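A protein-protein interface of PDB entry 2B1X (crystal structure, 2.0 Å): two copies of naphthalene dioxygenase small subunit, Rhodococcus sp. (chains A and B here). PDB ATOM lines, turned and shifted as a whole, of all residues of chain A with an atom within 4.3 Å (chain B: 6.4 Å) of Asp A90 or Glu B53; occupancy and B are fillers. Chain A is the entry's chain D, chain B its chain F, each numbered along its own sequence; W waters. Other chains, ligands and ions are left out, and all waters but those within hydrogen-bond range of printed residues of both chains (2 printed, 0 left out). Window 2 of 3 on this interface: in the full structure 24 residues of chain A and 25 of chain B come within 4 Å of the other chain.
NH1 of Arg B54 lies within hydrogen-bond range of O of Glu A89 (2.7 Å). The backbone NH of Arg B54 lies within hydrogen-bond range of the side-chain carboxylate of Asp A90 (2.9 Å).
Among the printed residues, merely in contact across the chains: Asp A90 with Glu B53, Pro A91 with Thr B51, Pro A91 with Arg B52, Pro A92 with Arg B52 and Pro A92 with Arg B54.
Ala A86 touches none of the printed residues of chain B. Ala A88 touches none of the printed residues of chain B. Of chain B, only Glu B53 (3.4 Å) and Arg B54 (2.9 Å) come within 4 Å of Asp A90. Of the printed residues of chain B, Pro A91 touches Thr B51 (3.5 Å) and Arg B52 (3.3 Å). Of the printed residues of chain A, Thr B51 touches Pro A91. Of chain A, only Asp A90 (3.4 Å) comes within 4 Å of Glu B53. The nearest residue of chain B that does not touch Asp A90 is Glu B55 (4.9 Å). The nearest residue of chain A that does not touch Glu B53 is Pro A92 (4.2 Å).
Of the 8 printed residues of chain A, 4 touch a printed residue of chain B. Printed residues of chain A that touch a printed residue of chain B: Glu A89, Asp A90, Pro A91 and Pro A92. Hydrophobic or aromatic side chains of chain A that line the printed part of chain B: Pro A91 and Pro A92. Of the 7 printed residues of chain B, 4 touch a printed residue of chain A. Printed residues of chain B that touch a printed residue of chain A: Thr B51, Arg B52, Glu B53 and Arg B54. Among the printed residues, 7 pairs touch across the chains.
No position is printed for both chains.
Water W2 bridges the side-chain carboxylate (OE1) of Glu A89 (2.6 Å) and the guanidinium group (NH2) of Arg B54 (3.0 Å). Water W1 lies within hydrogen-bond range of OD2 of Asp A90 (2.9 Å), N of Glu B55 (2.9 Å) and N of Arg B54 (3.4 Å).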
ATOM      1  N   GLU A  84      -5.612 -19.438  -0.421  1.00  0.00           N
ATOM      2  CA  GLU A  84      -4.635 -20.064   0.438  1.00  0.00           C
ATOM      3  C   GLU A  84      -5.023 -21.527   0.655  1.00  0.00           C
ATOM      4  O   GLU A  84      -4.445 -22.172   1.511  1.00  0.00           O
ATOM      5  CB  GLU A  84      -4.573 -19.323   1.782  1.00  0.00           C
ATOM      6  CG  GLU A  84      -3.904 -17.946   1.699  1.00  0.00           C
ATOM      7  CD  GLU A  84      -4.091 -17.077   2.946  1.00  0.00           C
ATOM      8  OE1 GLU A  84      -4.927 -17.406   3.832  1.00  0.00           O
ATOM      9  OE2 GLU A  84      -3.393 -16.037   3.066  1.00  0.00           O
ATOM     10  N   ALA A  86      -5.884 -24.098  -2.092  1.00  0.00           N
ATOM     11  CA  ALA A  86      -6.013 -24.994  -3.255  1.00  0.00           C
ATOM     12  C   ALA A  86      -5.089 -26.201  -3.049  1.00  0.00           C
ATOM     13  O   ALA A  86      -3.988 -26.251  -3.606  1.00  0.00           O
ATOM     14  CB  ALA A  86      -5.687 -24.256  -4.558  1.00  0.00           C
ATOM     15  N   TRP A  87      -5.554 -27.153  -2.246  1.00  0.00           N
ATOM     16  CA  TRP A  87      -4.702 -28.197  -1.677  1.00  0.00           C
ATOM     17  C   TRP A  87      -4.069 -29.095  -2.747  1.00  0.00           C
ATOM     18  O   TRP A  87      -2.965 -29.602  -2.549  1.00  0.00           O
ATOM     19  CB  TRP A  87      -5.468 -29.055  -0.649  1.00  0.00           C
ATOM     20  CG  TRP A  87      -6.310 -28.262   0.384  1.00  0.00           C
ATOM     21  CD1 TRP A  87      -7.667 -28.218   0.454  1.00  0.00           C
ATOM     22  CD2 TRP A  87      -5.827 -27.394   1.426  1.00  0.00           C
ATOM     23  NE1 TRP A  87      -8.060 -27.417   1.491  1.00  0.00           N
ATOM     24  CE2 TRP A  87      -6.949 -26.887   2.102  1.00  0.00           C
ATOM     25  CE3 TRP A  87      -4.552 -26.991   1.850  1.00  0.00           C
ATOM     26  CZ2 TRP A  87      -6.848 -25.987   3.166  1.00  0.00           C
ATOM     27  CZ3 TRP A  87      -4.434 -26.104   2.939  1.00  0.00           C
ATOM     28  CH2 TRP A  87      -5.580 -25.612   3.582  1.00  0.00           C
ATOM     29  N   ALA A  88      -4.763 -29.299  -3.865  1.00  0.00           N
ATOM     30  CA  ALA A  88      -4.244 -30.107  -4.946  1.00  0.00           C
ATOM     31  C   ALA A  88      -2.883 -29.539  -5.437  1.00  0.00           C
ATOM     32  O   ALA A  88      -2.028 -30.299  -5.872  1.00  0.00           O
ATOM     33  CB  ALA A  88      -5.242 -30.143  -6.106  1.00  0.00           C
ATOM     34  N   GLU A  89      -2.723 -28.220  -5.365  1.00  0.00           N
ATOM     35  CA  GLU A  89      -1.505 -27.535  -5.854  1.00  0.00           C
ATOM     36  C   GLU A  89      -0.899 -26.637  -4.785  1.00  0.00           C
ATOM     37  O   GLU A  89      -0.294 -25.612  -5.068  1.00  0.00           O
ATOM     38  CB  GLU A  89      -1.797 -26.749  -7.168  1.00  0.00           C
ATOM     39  CG  GLU A  89      -1.935 -27.706  -8.369  1.00  0.00           C
ATOM     40  CD  GLU A  89      -0.636 -28.468  -8.620  1.00  0.00           C
ATOM     41  OE1 GLU A  89       0.402 -27.789  -8.529  1.00  0.00           O
ATOM     42  OE2 GLU A  89      -0.628 -29.720  -8.898  1.00  0.00           O
ATOM     43  N   ASP A  90      -1.070 -27.017  -3.535  1.00  0.00           N
ATOM     44  CA  ASP A  90      -0.416 -26.284  -2.465  1.00  0.00           C
ATOM     45  C   ASP A  90      -0.113 -27.254  -1.352  1.00  0.00           C
ATOM     46  O   ASP A  90      -1.001 -27.541  -0.530  1.00  0.00           O
ATOM     47  CB  ASP A  90      -1.297 -25.129  -1.991  1.00  0.00           C
ATOM     48  CG  ASP A  90      -0.551 -24.153  -1.063  1.00  0.00           C
ATOM     49  OD1 ASP A  90       0.605 -24.471  -0.651  1.00  0.00           O
ATOM     50  OD2 ASP A  90      -1.059 -23.052  -0.703  1.00  0.00           O
ATOM     51  N   PRO A  91       1.110 -27.761  -1.260  1.00  0.00           N
ATOM     52  CA  PRO A  91       2.284 -27.395  -2.100  1.00  0.00           C
ATOM     53  C   PRO A  91       2.152 -27.658  -3.623  1.00  0.00           C
ATOM     54  O   PRO A  91       1.517 -28.631  -4.014  1.00  0.00           O
ATOM     55  CB  PRO A  91       3.392 -28.280  -1.544  1.00  0.00           C
ATOM     56  CG  PRO A  91       2.936 -28.645  -0.142  1.00  0.00           C
ATOM     57  CD  PRO A  91       1.431 -28.770  -0.234  1.00  0.00           C
ATOM     58  N   PRO A  92       2.774 -26.814  -4.446  1.00  0.00           N
ATOM     59  CA  PRO A  92       2.677 -26.943  -5.913  1.00  0.00           C
ATOM     60  C   PRO A  92       3.426 -28.164  -6.413  1.00  0.00           C
ATOM     61  O   PRO A  92       4.431 -28.578  -5.821  1.00  0.00           O
ATOM     62  CB  PRO A  92       3.340 -25.662  -6.447  1.00  0.00           C
ATOM     63  CG  PRO A  92       4.223 -25.195  -5.345  1.00  0.00           C
ATOM     64  CD  PRO A  92       3.538 -25.622  -4.030  1.00  0.00           C
ATOM     65  N   THR B  51      10.116 -29.568  -1.022  1.00  0.00           N
ATOM     66  CA  THR B  51       8.697 -29.249  -1.155  1.00  0.00           C
ATOM     67  C   THR B  51       8.334 -28.206  -0.118  1.00  0.00           C
ATOM     68  O   THR B  51       8.541 -28.418   1.077  1.00  0.00           O
ATOM     69  CB  THR B  51       7.810 -30.479  -0.847  1.00  0.00           C
ATOM     70  OG1 THR B  51       8.164 -31.569  -1.714  1.00  0.00           O
ATOM     71  CG2 THR B  51       6.336 -30.168  -1.193  1.00  0.00           C
ATOM     72  N   ARG B  52       7.739 -27.109  -0.579  1.00  0.00           N
ATOM     73  CA  ARG B  52       7.232 -26.105   0.340  1.00  0.00           C
ATOM     74  C   ARG B  52       5.860 -25.630  -0.094  1.00  0.00           C
ATOM     75  O   ARG B  52       5.507 -25.767  -1.249  1.00  0.00           O
ATOM     76  CB  ARG B  52       8.195 -24.919   0.377  1.00  0.00           C
ATOM     77  CG  ARG B  52       9.614 -25.355   0.655  1.00  0.00           C
ATOM     78  CD  ARG B  52      10.457 -24.401   1.416  1.00  0.00           C
ATOM     79  NE  ARG B  52       9.777 -23.670   2.489  1.00  0.00           N
ATOM     80  CZ  ARG B  52      10.084 -22.413   2.811  1.00  0.00           C
ATOM     81  NH1 ARG B  52      11.007 -21.741   2.124  1.00  0.00           N
ATOM     82  NH2 ARG B  52       9.423 -21.810   3.792  1.00  0.00           N
ATOM     83  N   GLU B  53       5.097 -25.057   0.843  1.00  0.00           N
ATOM     84  CA  GLU B  53       3.851 -24.369   0.499  1.00  0.00           C
ATOM     85  C   GLU B  53       4.071 -23.296  -0.583  1.00  0.00           C
ATOM     86  O   GLU B  53       5.178 -22.765  -0.749  1.00  0.00           O
ATOM     87  CB  GLU B  53       3.199 -23.752   1.752  1.00  0.00           C
ATOM     88  CG  GLU B  53       4.059 -22.723   2.481  1.00  0.00           C
ATOM     89  CD  GLU B  53       4.788 -23.314   3.686  1.00  0.00           C
ATOM     90  OE1 GLU B  53       5.202 -24.506   3.610  1.00  0.00           O
ATOM     91  OE2 GLU B  53       4.966 -22.598   4.715  1.00  0.00           O
ATOM     92  N   ARG B  54       2.998 -22.991  -1.298  1.00  0.00           N
ATOM     93  CA  ARG B  54       3.027 -22.063  -2.424  1.00  0.00           C
ATOM     94  C   ARG B  54       3.534 -20.674  -1.985  1.00  0.00           C
ATOM     95  O   ARG B  54       4.233 -19.993  -2.732  1.00  0.00           O
ATOM     96  CB  ARG B  54       1.620 -21.993  -3.050  1.00  0.00           C
ATOM     97  CG  ARG B  54       1.472 -21.138  -4.279  1.00  0.00           C
ATOM     98  CD  ARG B  54       0.334 -21.584  -5.217  1.00  0.00           C
ATOM     99  NE  ARG B  54       0.913 -21.717  -6.544  1.00  0.00           N
ATOM    100  CZ  ARG B  54       0.839 -22.760  -7.340  1.00  0.00           C
ATOM    101  NH1 ARG B  54       0.163 -23.849  -7.027  1.00  0.00           N
ATOM    102  NH2 ARG B  54       1.460 -22.683  -8.504  1.00  0.00           N
ATOM    103  N   GLU B  55       3.212 -20.314  -0.751  1.00  0.00           N
ATOM    104  CA  GLU B  55       3.567 -19.029  -0.140  1.00  0.00           C
ATOM    105  C   GLU B  55       5.076 -18.767   0.005  1.00  0.00           C
ATOM    106  O   GLU B  55       5.517 -17.610  -0.022  1.00  0.00           O
ATOM    107  CB  GLU B  55       2.963 -18.976   1.242  1.00  0.00           C
ATOM    108  CG  GLU B  55       2.259 -17.692   1.548  1.00  0.00           C
ATOM    109  CD  GLU B  55       1.682 -17.693   2.946  1.00  0.00           C
ATOM    110  OE1 GLU B  55       0.429 -17.594   3.059  1.00  0.00           O
ATOM    111  OE2 GLU B  55       2.479 -17.801   3.920  1.00  0.00           O
ATOM    112  N   ALA B  56       5.856 -19.835   0.179  1.00  0.00           N
ATOM    113  CA  ALA B  56       7.302 -19.732   0.302  1.00  0.00           C
ATOM    114  C   ALA B  56       7.884 -18.957  -0.880  1.00  0.00           C
ATOM    115  O   ALA B  56       7.477 -19.146  -2.011  1.00  0.00           O
ATOM    116  CB  ALA B  56       7.948 -21.120   0.415  1.00  0.00           C
ATOM    117  N   VAL B  57       8.818 -18.068  -0.591  1.00  0.00           N
ATOM    118  CA  VAL B  57       9.483 -17.256  -1.619  1.00  0.00           C
ATOM    119  C   VAL B  57      10.312 -18.115  -2.562  1.00  0.00           C
ATOM    120  O   VAL B  57      10.394 -17.844  -3.779  1.00  0.00           O
ATOM    121  CB  VAL B  57      10.366 -16.129  -0.968  1.00  0.00           C
ATOM    122  CG1 VAL B  57      11.245 -15.428  -1.996  1.00  0.00           C
ATOM    123  CG2 VAL B  57       9.477 -15.096  -0.271  1.00  0.00           C
HETATM  124  O   HOH W   1       0.763 -21.203   0.577  1.00  0.00           O
HETATM  125  O   HOH W   2       0.911 -25.435  -9.602  1.00  0.00           O
